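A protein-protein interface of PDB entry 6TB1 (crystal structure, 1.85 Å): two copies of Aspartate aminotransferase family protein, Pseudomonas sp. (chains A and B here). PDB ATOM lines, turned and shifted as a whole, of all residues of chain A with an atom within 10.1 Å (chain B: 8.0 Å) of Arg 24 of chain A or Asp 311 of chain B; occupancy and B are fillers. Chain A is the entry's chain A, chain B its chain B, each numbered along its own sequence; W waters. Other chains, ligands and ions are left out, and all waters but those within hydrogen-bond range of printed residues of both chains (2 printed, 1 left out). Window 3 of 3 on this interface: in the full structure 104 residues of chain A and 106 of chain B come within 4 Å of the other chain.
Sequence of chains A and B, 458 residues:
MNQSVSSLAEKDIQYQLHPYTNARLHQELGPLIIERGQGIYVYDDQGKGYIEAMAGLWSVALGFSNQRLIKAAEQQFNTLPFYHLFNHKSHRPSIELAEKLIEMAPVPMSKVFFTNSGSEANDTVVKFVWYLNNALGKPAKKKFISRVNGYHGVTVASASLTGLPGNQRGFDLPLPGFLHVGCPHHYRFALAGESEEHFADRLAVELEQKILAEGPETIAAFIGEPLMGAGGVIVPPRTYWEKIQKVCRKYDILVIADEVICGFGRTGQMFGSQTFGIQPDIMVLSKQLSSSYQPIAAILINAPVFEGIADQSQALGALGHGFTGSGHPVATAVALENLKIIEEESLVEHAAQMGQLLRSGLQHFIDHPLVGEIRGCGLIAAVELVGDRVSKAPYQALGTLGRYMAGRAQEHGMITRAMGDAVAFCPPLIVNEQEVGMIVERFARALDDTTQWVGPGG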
ATOM      1  N   ILE A  13       5.566  17.608  -7.718  1.00  0.00           N
ATOM      2  CA  ILE A  13       5.045  18.854  -8.354  1.00  0.00           C
ATOM      3  C   ILE A  13       6.190  19.587  -9.058  1.00  0.00           C
ATOM      4  O   ILE A  13       5.970  20.131 -10.172  1.00  0.00           O
ATOM      5  CB  ILE A  13       4.347  19.764  -7.314  1.00  0.00           C
ATOM      6  CG1 ILE A  13       2.984  19.198  -6.919  1.00  0.00           C
ATOM      7  CG2 ILE A  13       4.225  21.194  -7.825  1.00  0.00           C
ATOM      8  CD1 ILE A  13       2.476  19.686  -5.583  1.00  0.00           C
ATOM      9  N   GLN A  16       7.986  16.354 -12.114  1.00  0.00           N
ATOM     10  CA  GLN A  16       7.322  15.369 -13.029  1.00  0.00           C
ATOM     11  C   GLN A  16       6.197  15.995 -13.859  1.00  0.00           C
ATOM     12  O   GLN A  16       5.249  16.564 -13.258  1.00  0.00           O
ATOM     13  CB  GLN A  16       6.753  14.177 -12.262  1.00  0.00           C
ATOM     14  CG  GLN A  16       7.820  13.269 -11.689  1.00  0.00           C
ATOM     15  CD  GLN A  16       7.418  11.809 -11.742  1.00  0.00           C
ATOM     16  OE1 GLN A  16       7.672  11.102 -12.720  1.00  0.00           O
ATOM     17  NE2 GLN A  16       6.773  11.352 -10.680  1.00  0.00           N
ATOM     18  N   LEU A  17       6.243  15.829 -15.193  1.00  0.00           N
ATOM     19  CA  LEU A  17       5.065  16.056 -16.081  1.00  0.00           C
ATOM     20  C   LEU A  17       4.264  14.744 -16.146  1.00  0.00           C
ATOM     21  O   LEU A  17       4.820  13.738 -16.657  1.00  0.00           O
ATOM     22  CB  LEU A  17       5.531  16.481 -17.474  1.00  0.00           C
ATOM     23  CG  LEU A  17       4.452  16.747 -18.513  1.00  0.00           C
ATOM     24  CD1 LEU A  17       3.566  17.910 -18.095  1.00  0.00           C
ATOM     25  CD2 LEU A  17       5.067  17.036 -19.889  1.00  0.00           C
ATOM     26  N   HIS A  18       3.014  14.748 -15.685  1.00  0.00           N
ATOM     27  CA  HIS A  18       2.177  13.519 -15.619  1.00  0.00           C
ATOM     28  C   HIS A  18       1.427  13.270 -16.929  1.00  0.00           C
ATOM     29  O   HIS A  18       0.766  14.156 -17.489  1.00  0.00           O
ATOM     30  CB  HIS A  18       1.222  13.523 -14.408  1.00  0.00           C
ATOM     31  CG  HIS A  18       1.885  13.172 -13.123  1.00  0.00           C
ATOM     32  ND1 HIS A  18       1.765  11.909 -12.544  1.00  0.00           N
ATOM     33  CD2 HIS A  18       2.717  13.888 -12.319  1.00  0.00           C
ATOM     34  CE1 HIS A  18       2.500  11.869 -11.438  1.00  0.00           C
ATOM     35  NE2 HIS A  18       3.096  13.072 -11.278  1.00  0.00           N
ATOM     36  N   TYR A  20      -1.854  12.067 -18.971  1.00  0.00           N
ATOM     37  CA  TYR A  20      -3.322  12.007 -18.800  1.00  0.00           C
ATOM     38  C   TYR A  20      -3.708  12.821 -17.553  1.00  0.00           C
ATOM     39  O   TYR A  20      -4.593  12.405 -16.777  1.00  0.00           O
ATOM     40  CB  TYR A  20      -3.740  10.533 -18.790  1.00  0.00           C
ATOM     41  CG  TYR A  20      -3.724   9.860 -20.145  1.00  0.00           C
ATOM     42  CD1 TYR A  20      -4.621  10.241 -21.135  1.00  0.00           C
ATOM     43  CD2 TYR A  20      -2.851   8.815 -20.435  1.00  0.00           C
ATOM     44  CE1 TYR A  20      -4.648   9.609 -22.371  1.00  0.00           C
ATOM     45  CE2 TYR A  20      -2.858   8.184 -21.672  1.00  0.00           C
ATOM     46  CZ  TYR A  20      -3.769   8.569 -22.641  1.00  0.00           C
ATOM     47  OH  TYR A  20      -3.805   7.919 -23.851  1.00  0.00           O
ATOM     48  N   THR A  21      -3.104  14.011 -17.405  1.00  0.00           N
ATOM     49  CA  THR A  21      -3.277  14.911 -16.236  1.00  0.00           C
ATOM     50  C   THR A  21      -3.339  16.376 -16.707  1.00  0.00           C
ATOM     51  O   THR A  21      -2.609  16.728 -17.653  1.00  0.00           O
ATOM     52  CB  THR A  21      -2.170  14.674 -15.198  1.00  0.00           C
ATOM     53  OG1 THR A  21      -2.134  13.294 -14.800  1.00  0.00           O
ATOM     54  CG2 THR A  21      -2.322  15.542 -13.963  1.00  0.00           C
ATOM     55  N   ASN A  22      -4.179  17.186 -16.054  1.00  0.00           N
ATOM     56  CA  ASN A  22      -4.187  18.679 -16.152  1.00  0.00           C
ATOM     57  C   ASN A  22      -2.961  19.186 -15.373  1.00  0.00           C
ATOM     58  O   ASN A  22      -2.967  19.105 -14.126  1.00  0.00           O
ATOM     59  CB  ASN A  22      -5.524  19.262 -15.658  1.00  0.00           C
ATOM     60  CG  ASN A  22      -5.573  20.778 -15.586  1.00  0.00           C
ATOM     61  OD1 ASN A  22      -4.531  21.434 -15.531  1.00  0.00           O
ATOM     62  ND2 ASN A  22      -6.788  21.339 -15.570  1.00  0.00           N
ATOM     63  N   ALA A  23      -1.918  19.655 -16.061  1.00  0.00           N
ATOM     64  CA  ALA A  23      -0.618  19.982 -15.425  1.00  0.00           C
ATOM     65  C   ALA A  23      -0.780  21.152 -14.435  1.00  0.00           C
ATOM     66  O   ALA A  23      -0.024  21.186 -13.451  1.00  0.00           O
ATOM     67  CB  ALA A  23       0.420  20.282 -16.470  1.00  0.00           C
ATOM     68  N   ARG A  24      -1.673  22.100 -14.710  1.00  0.00           N
ATOM     69  CA  ARG A  24      -1.903  23.287 -13.830  1.00  0.00           C
ATOM     70  C   ARG A  24      -2.649  22.849 -12.562  1.00  0.00           C
ATOM     71  O   ARG A  24      -2.221  23.215 -11.465  1.00  0.00           O
ATOM     72  CB  ARG A  24      -2.649  24.389 -14.594  1.00  0.00           C
ATOM     73  CG  ARG A  24      -1.850  25.015 -15.737  1.00  0.00           C
ATOM     74  CD  ARG A  24      -0.485  25.520 -15.304  1.00  0.00           C
ATOM     75  NE  ARG A  24       0.129  26.418 -16.277  1.00  0.00           N
ATOM     76  CZ  ARG A  24       1.418  26.781 -16.287  1.00  0.00           C
ATOM     77  NH1 ARG A  24       2.269  26.293 -15.397  1.00  0.00           N
ATOM     78  NH2 ARG A  24       1.847  27.622 -17.217  1.00  0.00           N
ATOM     79  N   LEU A  25      -3.703  22.045 -12.692  1.00  0.00           N
ATOM     80  CA  LEU A  25      -4.419  21.482 -11.518  1.00  0.00           C
ATOM     81  C   LEU A  25      -3.438  20.643 -10.693  1.00  0.00           C
ATOM     82  O   LEU A  25      -3.480  20.718  -9.452  1.00  0.00           O
ATOM     83  CB  LEU A  25      -5.619  20.659 -12.010  1.00  0.00           C
ATOM     84  CG  LEU A  25      -6.519  20.096 -10.902  1.00  0.00           C
ATOM     85  CD1 LEU A  25      -7.095  21.223 -10.033  1.00  0.00           C
ATOM     86  CD2 LEU A  25      -7.650  19.275 -11.510  1.00  0.00           C
ATOM     87  N   HIS A  26      -2.515  19.930 -11.348  1.00  0.00           N
ATOM     88  CA  HIS A  26      -1.495  19.108 -10.659  1.00  0.00           C
ATOM     89  C   HIS A  26      -0.614  20.005  -9.768  1.00  0.00           C
ATOM     90  O   HIS A  26      -0.249  19.564  -8.649  1.00  0.00           O
ATOM     91  CB  HIS A  26      -0.666  18.268 -11.648  1.00  0.00           C
ATOM     92  CG  HIS A  26       0.164  17.254 -10.941  1.00  0.00           C
ATOM     93  ND1 HIS A  26      -0.418  16.155 -10.343  1.00  0.00           N
ATOM     94  CD2 HIS A  26       1.497  17.171 -10.699  1.00  0.00           C
ATOM     95  CE1 HIS A  26       0.514  15.448  -9.739  1.00  0.00           C
ATOM     96  NE2 HIS A  26       1.707  16.052  -9.934  1.00  0.00           N
ATOM     97  N   GLN A  27      -0.220  21.188 -10.253  1.00  0.00           N
ATOM     98  CA  GLN A  27       0.659  22.111  -9.484  1.00  0.00           C
ATOM     99  C   GLN A  27      -0.071  22.586  -8.221  1.00  0.00           C
ATOM    100  O   GLN A  27       0.614  22.797  -7.208  1.00  0.00           O
ATOM    101  CB  GLN A  27       1.099  23.287 -10.358  1.00  0.00           C
ATOM    102  CG  GLN A  27       2.104  22.871 -11.434  1.00  0.00           C
ATOM    103  CD  GLN A  27       2.541  24.049 -12.265  1.00  0.00           C
ATOM    104  OE1 GLN A  27       1.720  24.721 -12.890  1.00  0.00           O
ATOM    105  NE2 GLN A  27       3.847  24.294 -12.271  1.00  0.00           N
ATOM    106  N   GLU A  28      -1.400  22.675  -8.263  1.00  0.00           N
ATOM    107  CA  GLU A  28      -2.228  23.060  -7.087  1.00  0.00           C
ATOM    108  C   GLU A  28      -2.437  21.868  -6.144  1.00  0.00           C
ATOM    109  O   GLU A  28      -2.160  22.026  -4.951  1.00  0.00           O
ATOM    110  CB  GLU A  28      -3.554  23.648  -7.551  1.00  0.00           C
ATOM    111  CG  GLU A  28      -4.308  24.351  -6.433  1.00  0.00           C
ATOM    112  CD  GLU A  28      -5.762  24.627  -6.759  1.00  0.00           C
ATOM    113  OE1 GLU A  28      -6.054  24.898  -7.942  1.00  0.00           O
ATOM    114  OE2 GLU A  28      -6.592  24.567  -5.833  1.00  0.00           O
ATOM    115  N   LEU A  29      -2.906  20.714  -6.635  1.00  0.00           N
ATOM    116  CA  LEU A  29      -3.391  19.607  -5.763  1.00  0.00           C
ATOM    117  C   LEU A  29      -2.276  18.619  -5.436  1.00  0.00           C
ATOM    118  O   LEU A  29      -2.363  17.973  -4.369  1.00  0.00           O
ATOM    119  CB  LEU A  29      -4.540  18.861  -6.454  1.00  0.00           C
ATOM    120  CG  LEU A  29      -5.793  19.672  -6.773  1.00  0.00           C
ATOM    121  CD1 LEU A  29      -6.873  18.761  -7.338  1.00  0.00           C
ATOM    122  CD2 LEU A  29      -6.310  20.422  -5.554  1.00  0.00           C
ATOM    123  N   GLY A  30      -1.300  18.446  -6.336  1.00  0.00           N
ATOM    124  CA  GLY A  30      -0.228  17.464  -6.141  1.00  0.00           C
ATOM    125  C   GLY A  30      -0.733  16.038  -6.384  1.00  0.00           C
ATOM    126  O   GLY A  30      -1.884  15.819  -6.759  1.00  0.00           O
ATOM    127  N   PRO A  31       0.147  15.030  -6.226  1.00  0.00           N
ATOM    128  CA  PRO A  31      -0.200  13.641  -6.529  1.00  0.00           C
ATOM    129  C   PRO A  31      -0.987  12.904  -5.436  1.00  0.00           C
ATOM    130  O   PRO A  31      -1.012  13.354  -4.304  1.00  0.00           O
ATOM    131  CB  PRO A  31       1.171  12.980  -6.668  1.00  0.00           C
ATOM    132  CG  PRO A  31       2.048  13.770  -5.715  1.00  0.00           C
ATOM    133  CD  PRO A  31       1.555  15.189  -5.853  1.00  0.00           C
ATOM    134  N   ARG A 403     -16.701  11.937 -13.692  1.00  0.00           N
ATOM    135  CA  ARG A 403     -15.611  12.499 -12.860  1.00  0.00           C
ATOM    136  C   ARG A 403     -16.000  12.418 -11.382  1.00  0.00           C
ATOM    137  O   ARG A 403     -15.158  11.974 -10.536  1.00  0.00           O
ATOM    138  CB  ARG A 403     -15.315  13.936 -13.291  1.00  0.00           C
ATOM    139  CG  ARG A 403     -14.029  14.497 -12.704  1.00  0.00           C
ATOM    140  CD  ARG A 403     -13.992  16.019 -12.895  1.00  0.00           C
ATOM    141  NE  ARG A 403     -12.649  16.532 -12.656  1.00  0.00           N
ATOM    142  CZ  ARG A 403     -12.165  16.905 -11.480  1.00  0.00           C
ATOM    143  NH1 ARG A 403     -10.924  17.361 -11.400  1.00  0.00           N
ATOM    144  NH2 ARG A 403     -12.896  16.826 -10.380  1.00  0.00           N
ATOM    145  N   HIS B  88      -2.899  12.131 -11.988  1.00  0.00           N
ATOM    146  CA  HIS B  88      -2.289  12.584 -10.700  1.00  0.00           C
ATOM    147  C   HIS B  88      -1.700  11.425  -9.864  1.00  0.00           C
ATOM    148  O   HIS B  88      -1.116  11.724  -8.804  1.00  0.00           O
ATOM    149  CB  HIS B  88      -3.284  13.379  -9.830  1.00  0.00           C
ATOM    150  CG  HIS B  88      -3.945  14.529 -10.508  1.00  0.00           C
ATOM    151  ND1 HIS B  88      -3.348  15.757 -10.581  1.00  0.00           N
ATOM    152  CD2 HIS B  88      -5.165  14.659 -11.089  1.00  0.00           C
ATOM    153  CE1 HIS B  88      -4.157  16.602 -11.214  1.00  0.00           C
ATOM    154  NE2 HIS B  88      -5.280  15.944 -11.540  1.00  0.00           N
ATOM    155  N   LYS B 111      11.098  19.832 -16.112  1.00  0.00           N
ATOM    156  CA  LYS B 111      10.311  18.590 -15.857  1.00  0.00           C
ATOM    157  C   LYS B 111      10.872  17.384 -16.627  1.00  0.00           C
ATOM    158  O   LYS B 111      11.484  17.562 -17.692  1.00  0.00           O
ATOM    159  CB  LYS B 111       8.851  18.784 -16.282  1.00  0.00           C
ATOM    160  CG  LYS B 111       8.100  19.923 -15.590  1.00  0.00           C
ATOM    161  CD  LYS B 111       7.807  19.673 -14.118  1.00  0.00           C
ATOM    162  CE  LYS B 111       7.254  20.899 -13.410  1.00  0.00           C
ATOM    163  NZ  LYS B 111       8.297  21.952 -13.266  1.00  0.00           N
ATOM    164  N   TYR B 131       2.202  20.168 -30.101  1.00  0.00           N
ATOM    165  CA  TYR B 131       1.251  20.600 -29.030  1.00  0.00           C
ATOM    166  C   TYR B 131       1.632  22.004 -28.544  1.00  0.00           C
ATOM    167  O   TYR B 131       0.740  22.886 -28.464  1.00  0.00           O
ATOM    168  CB  TYR B 131       1.270  19.564 -27.905  1.00  0.00           C
ATOM    169  CG  TYR B 131       0.134  19.545 -26.907  1.00  0.00           C
ATOM    170  CD1 TYR B 131      -1.055  18.878 -27.177  1.00  0.00           C
ATOM    171  CD2 TYR B 131       0.321  20.018 -25.613  1.00  0.00           C
ATOM    172  CE1 TYR B 131      -2.057  18.760 -26.221  1.00  0.00           C
ATOM    173  CE2 TYR B 131      -0.666  19.889 -24.647  1.00  0.00           C
ATOM    174  CZ  TYR B 131      -1.868  19.273 -24.952  1.00  0.00           C
ATOM    175  OH  TYR B 131      -2.826  19.166 -23.968  1.00  0.00           O
ATOM    176  N   ALA B 135      -0.313  25.583 -28.849  1.00  0.00           N
ATOM    177  CA  ALA B 135      -0.604  26.337 -27.607  1.00  0.00           C
ATOM    178  C   ALA B 135      -0.163  27.805 -27.746  1.00  0.00           C
ATOM    179  O   ALA B 135      -0.814  28.680 -27.143  1.00  0.00           O
ATOM    180  CB  ALA B 135       0.071  25.708 -26.422  1.00  0.00           C
ATOM    181  N   LEU B 136       0.931  28.072 -28.463  1.00  0.00           N
ATOM    182  CA  LEU B 136       1.521  29.432 -28.570  1.00  0.00           C
ATOM    183  C   LEU B 136       0.871  30.199 -29.734  1.00  0.00           C
ATOM    184  O   LEU B 136       1.279  31.353 -29.968  1.00  0.00           O
ATOM    185  CB  LEU B 136       3.038  29.314 -28.756  1.00  0.00           C
ATOM    186  CG  LEU B 136       3.827  28.758 -27.566  1.00  0.00           C
ATOM    187  CD1 LEU B 136       5.317  28.686 -27.886  1.00  0.00           C
ATOM    188  CD2 LEU B 136       3.617  29.577 -26.303  1.00  0.00           C
ATOM    189  N   ALA B 303      11.847  25.307 -19.080  1.00  0.00           N
ATOM    190  CA  ALA B 303      10.676  26.084 -18.598  1.00  0.00           C
ATOM    191  C   ALA B 303       9.752  26.479 -19.743  1.00  0.00           C
ATOM    192  O   ALA B 303       8.543  26.211 -19.683  1.00  0.00           O
ATOM    193  CB  ALA B 303      11.148  27.290 -17.801  1.00  0.00           C
ATOM    194  N   PRO B 304      10.233  27.136 -20.829  1.00  0.00           N
ATOM    195  CA  PRO B 304       9.348  27.543 -21.918  1.00  0.00           C
ATOM    196  C   PRO B 304       8.555  26.383 -22.550  1.00  0.00           C
ATOM    197  O   PRO B 304       7.354  26.534 -22.836  1.00  0.00           O
ATOM    198  CB  PRO B 304      10.243  28.194 -22.979  1.00  0.00           C
ATOM    199  CG  PRO B 304      11.650  28.046 -22.468  1.00  0.00           C
ATOM    200  CD  PRO B 304      11.601  27.619 -21.020  1.00  0.00           C
ATOM    201  N   VAL B 305       9.210  25.238 -22.764  1.00  0.00           N
ATOM    202  CA  VAL B 305       8.513  24.058 -23.354  1.00  0.00           C
ATOM    203  C   VAL B 305       7.410  23.589 -22.383  1.00  0.00           C
ATOM    204  O   VAL B 305       6.262  23.367 -22.846  1.00  0.00           O
ATOM    205  CB  VAL B 305       9.524  22.952 -23.718  1.00  0.00           C
ATOM    206  CG1 VAL B 305       8.819  21.682 -24.173  1.00  0.00           C
ATOM    207  CG2 VAL B 305      10.491  23.422 -24.796  1.00  0.00           C
ATOM    208  N   PHE B 306       7.727  23.440 -21.093  1.00  0.00           N
ATOM    209  CA  PHE B 306       6.757  22.968 -20.061  1.00  0.00           C
ATOM    210  C   PHE B 306       5.576  23.949 -19.944  1.00  0.00           C
ATOM    211  O   PHE B 306       4.401  23.515 -19.947  1.00  0.00           O
ATOM    212  CB  PHE B 306       7.407  22.782 -18.686  1.00  0.00           C
ATOM    213  CG  PHE B 306       6.394  22.637 -17.574  1.00  0.00           C
ATOM    214  CD1 PHE B 306       5.546  21.531 -17.512  1.00  0.00           C
ATOM    215  CD2 PHE B 306       6.213  23.650 -16.645  1.00  0.00           C
ATOM    216  CE1 PHE B 306       4.585  21.426 -16.512  1.00  0.00           C
ATOM    217  CE2 PHE B 306       5.254  23.536 -15.643  1.00  0.00           C
ATOM    218  CZ  PHE B 306       4.445  22.425 -15.577  1.00  0.00           C
ATOM    219  N   GLU B 307       5.853  25.252 -19.830  1.00  0.00           N
ATOM    220  CA  GLU B 307       4.782  26.248 -19.532  1.00  0.00           C
ATOM    221  C   GLU B 307       3.720  26.233 -20.645  1.00  0.00           C
ATOM    222  O   GLU B 307       2.508  26.280 -20.319  1.00  0.00           O
ATOM    223  CB  GLU B 307       5.382  27.645 -19.312  1.00  0.00           C
ATOM    224  CG  GLU B 307       6.293  27.718 -18.103  1.00  0.00           C
ATOM    225  CD  GLU B 307       5.692  27.507 -16.727  1.00  0.00           C
ATOM    226  OE1 GLU B 307       4.481  27.764 -16.551  1.00  0.00           O
ATOM    227  OE2 GLU B 307       6.437  27.084 -15.836  1.00  0.00           O
ATOM    228  N   GLY B 308       4.130  26.127 -21.912  1.00  0.00           N
ATOM    229  CA  GLY B 308       3.188  26.084 -23.044  1.00  0.00           C
ATOM    230  C   GLY B 308       2.365  24.800 -23.062  1.00  0.00           C
ATOM    231  O   GLY B 308       1.139  24.864 -23.283  1.00  0.00           O
ATOM    232  N   ILE B 309       3.003  23.648 -22.833  1.00  0.00           N
ATOM    233  CA  ILE B 309       2.292  22.336 -22.743  1.00  0.00           C
ATOM    234  C   ILE B 309       1.289  22.395 -21.571  1.00  0.00           C
ATOM    235  O   ILE B 309       0.134  21.956 -21.748  1.00  0.00           O
ATOM    236  CB  ILE B 309       3.312  21.176 -22.605  1.00  0.00           C
ATOM    237  CG1 ILE B 309       4.161  21.032 -23.872  1.00  0.00           C
ATOM    238  CG2 ILE B 309       2.605  19.885 -22.245  1.00  0.00           C
ATOM    239  CD1 ILE B 309       5.370  20.135 -23.725  1.00  0.00           C
ATOM    240  N   ALA B 310       1.703  22.927 -20.416  1.00  0.00           N
ATOM    241  CA  ALA B 310       0.872  22.981 -19.190  1.00  0.00           C
ATOM    242  C   ALA B 310      -0.402  23.818 -19.450  1.00  0.00           C
ATOM    243  O   ALA B 310      -1.507  23.358 -19.083  1.00  0.00           O
ATOM    244  CB  ALA B 310       1.693  23.502 -18.034  1.00  0.00           C
ATOM    245  N   ASP B 311      -0.262  24.976 -20.100  1.00  0.00           N
ATOM    246  CA  ASP B 311      -1.405  25.864 -20.472  1.00  0.00           C
ATOM    247  C   ASP B 311      -2.403  25.107 -21.355  1.00  0.00           C
ATOM    248  O   ASP B 311      -3.626  25.152 -21.074  1.00  0.00           O
ATOM    249  CB  ASP B 311      -0.921  27.130 -21.185  1.00  0.00           C
ATOM    250  CG  ASP B 311      -0.371  28.202 -20.267  1.00  0.00           C
ATOM    251  OD1 ASP B 311      -0.517  28.063 -19.041  1.00  0.00           O
ATOM    252  OD2 ASP B 311       0.183  29.178 -20.794  1.00  0.00           O
ATOM    253  N   GLN B 312      -1.921  24.430 -22.396  1.00  0.00           N
ATOM    254  CA  GLN B 312      -2.807  23.700 -23.333  1.00  0.00           C
ATOM    255  C   GLN B 312      -3.488  22.521 -22.607  1.00  0.00           C
ATOM    256  O   GLN B 312      -4.671  22.261 -22.916  1.00  0.00           O
ATOM    257  CB  GLN B 312      -2.043  23.262 -24.582  1.00  0.00           C
ATOM    258  CG  GLN B 312      -2.990  22.699 -25.637  1.00  0.00           C
ATOM    259  CD  GLN B 312      -2.530  22.874 -27.058  1.00  0.00           C
ATOM    260  OE1 GLN B 312      -1.786  22.059 -27.597  1.00  0.00           O
ATOM    261  NE2 GLN B 312      -3.038  23.903 -27.696  1.00  0.00           N
ATOM    262  N   SER B 313      -2.794  21.839 -21.681  1.00  0.00           N
ATOM    263  CA  SER B 313      -3.342  20.662 -20.931  1.00  0.00           C
ATOM    264  C   SER B 313      -4.522  21.115 -20.048  1.00  0.00           C
ATOM    265  O   SER B 313      -5.467  20.316 -19.857  1.00  0.00           O
ATOM    266  CB  SER B 313      -2.291  19.955 -20.110  1.00  0.00           C
ATOM    267  OG  SER B 313      -1.948  20.675 -18.920  1.00  0.00           O
ATOM    268  N   GLN B 314      -4.473  22.354 -19.552  1.00  0.00           N
ATOM    269  CA  GLN B 314      -5.565  22.975 -18.758  1.00  0.00           C
ATOM    270  C   GLN B 314      -6.752  23.266 -19.682  1.00  0.00           C
ATOM    271  O   GLN B 314      -7.864  22.797 -19.381  1.00  0.00           O
ATOM    272  CB  GLN B 314      -5.024  24.224 -18.065  1.00  0.00           C
ATOM    273  CG  GLN B 314      -6.045  25.033 -17.282  1.00  0.00           C
ATOM    274  CD  GLN B 314      -5.324  26.184 -16.614  1.00  0.00           C
ATOM    275  OE1 GLN B 314      -4.670  26.995 -17.270  1.00  0.00           O
ATOM    276  NE2 GLN B 314      -5.375  26.224 -15.295  1.00  0.00           N
ATOM    277  N   ALA B 315      -6.509  23.967 -20.794  1.00  0.00           N
ATOM    278  CA  ALA B 315      -7.549  24.366 -21.769  1.00  0.00           C
ATOM    279  C   ALA B 315      -8.272  23.130 -22.330  1.00  0.00           C
ATOM    280  O   ALA B 315      -9.497  23.210 -22.509  1.00  0.00           O
ATOM    281  CB  ALA B 315      -6.930  25.196 -22.866  1.00  0.00           C
ATOM    282  N   LEU B 316      -7.566  22.031 -22.614  1.00  0.00           N
ATOM    283  CA  LEU B 316      -8.181  20.829 -23.250  1.00  0.00           C
ATOM    284  C   LEU B 316      -8.587  19.782 -22.199  1.00  0.00           C
ATOM    285  O   LEU B 316      -8.965  18.688 -22.611  1.00  0.00           O
ATOM    286  CB  LEU B 316      -7.204  20.220 -24.261  1.00  0.00           C
ATOM    287  CG  LEU B 316      -6.707  21.134 -25.381  1.00  0.00           C
ATOM    288  CD1 LEU B 316      -5.822  20.339 -26.329  1.00  0.00           C
ATOM    289  CD2 LEU B 316      -7.858  21.780 -26.138  1.00  0.00           C
ATOM    290  N   GLY B 317      -8.475  20.075 -20.905  1.00  0.00           N
ATOM    291  CA  GLY B 317      -8.948  19.191 -19.820  1.00  0.00           C
ATOM    292  C   GLY B 317      -7.846  18.326 -19.215  1.00  0.00           C
ATOM    293  O   GLY B 317      -7.792  18.219 -17.966  1.00  0.00           O
HETATM  294  O   HOH W   1      -6.875  24.048 -14.272  1.00  0.00           O
HETATM  295  O   HOH W   2       5.363  26.513 -13.458  1.00  0.00           O
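Of the 17 printed residues of chain A, 10 touch a printed residue of chain B. Hydrophobic or aromatic side chains of chain A that line the printed part of chain B: Leu 17, Ala 23, His 26 and Pro 31. Of the 20 printed residues of chain B, 9 touch a printed residue of chain A. Among the printed residues, 16 pairs touch across the chains.
The side-chain amide oxygen (OD1) of Asn 22 of chain A lies within hydrogen-bond range of the backbone NH (N) of Arg 24 of chain A (3.0 Å). The side-chain amide oxygen of Asn 22 of chain A lies within hydrogen-bond range of the backbone NH of Leu 25 of chain A (3.0 Å).
Among the printed residues, pairs that only touch across the chains: Ile 13 of chain A with Lys 111 of chain B (3.6 Å), Gln 16 of chain A with Lys 111 of chain B (3.9 Å), Leu 17 of chain A with Phe 306 of chain B (3.99 Å), Asn 22 of chain A with Ser 313 of chain B (3.98 Å), Asn 22 of chain A with Gln 314 of chain B (3.7 Å), Asn 22 of chain A with Gly 317 of chain B (3.4 Å), Ala 23 of chain A with Ala 310 of chain B (3.8 Å), Arg 24 of chain A with Ala 310 of chain B (3.7 Å), Arg 24 of chain A with Gln 314 of chain B (3.4 Å), Gln 27 of chain A with Phe 306 of chain B (3.7 Å) and Pro 31 of chain A with His 88 of chain B (3.1 Å).
The backbone NH (N) of His 88 of chain B is in hydrogen-bond range of the side-chain hydroxyl (OG1) of Thr 21 of chain A, 3.1 Å away. The backbone NH (N) of Ala 23 of chain A sits at hydrogen-bond distance from the side-chain hydroxyl (OG) of Ser 313 of chain B (3.0 Å). The side-chain carboxylate of Glu 307 of chain B is in salt-bridge range of the guanidinium group of Arg 24 of chain A, 2.7 Å away. NH2 of Arg 24 of chain A is in salt-bridge range of OD1 of Asp 311 of chain B, at 3.0 Å. A ring nitrogen (ND1) of His 88 of chain B is in hydrogen-bond range of a ring nitrogen (ND1) of His 26 of chain A, 3.0 Å away.
No position is printed for both chains. Of the 16 pairs that touch across the chains among the printed residues, none has its exchanged pair printed and touching as well.
Water W2 bridges the side-chain carboxylate of Glu 307 of chain B (2.7 Å) and the side-chain amide nitrogen of Gln 27 of chain A (2.9 Å). Water W1 lies within hydrogen-bond range of the side-chain amide nitrogen (NE2) of Gln 314 of chain B (2.8 Å) and the side-chain amide nitrogen (ND2) of Asn 22 of chain A (3.0 Å).
Of chain B, only Glu 307, Ala 310, Asp 311 and Gln 314 come within 4 Å of Arg 24 of chain A. Printed residues of chain B within 4 Å of Ala 23 of chain A: Ala 310 and Ser 313. Of the printed residues of chain A, Glu 307 of chain B touches Arg 24. Ala 310 of chain B touches two residues of chain A. Ser 313 of chain B touches just these residues of chain A: Asn 22 (3.98 Å) and Ala 23 (3.0 Å). Of the printed residues of chain A, Phe 306 of chain B touches Leu 17 and Gln 27. Printed residues of chain B within 4 Å of Leu 17 of chain A: Phe 306. Of the printed residues of chain B, Ile 13 of chain A touches Lys 111. The nearest residue of chain A that does not touch Asp 311 of chain B is Ala 23 of chain A (6.0 Å). The nearest printed residue of chain B that does not touch Gln 27 of chain A is Lys 111 of chain B (4.9 Å).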
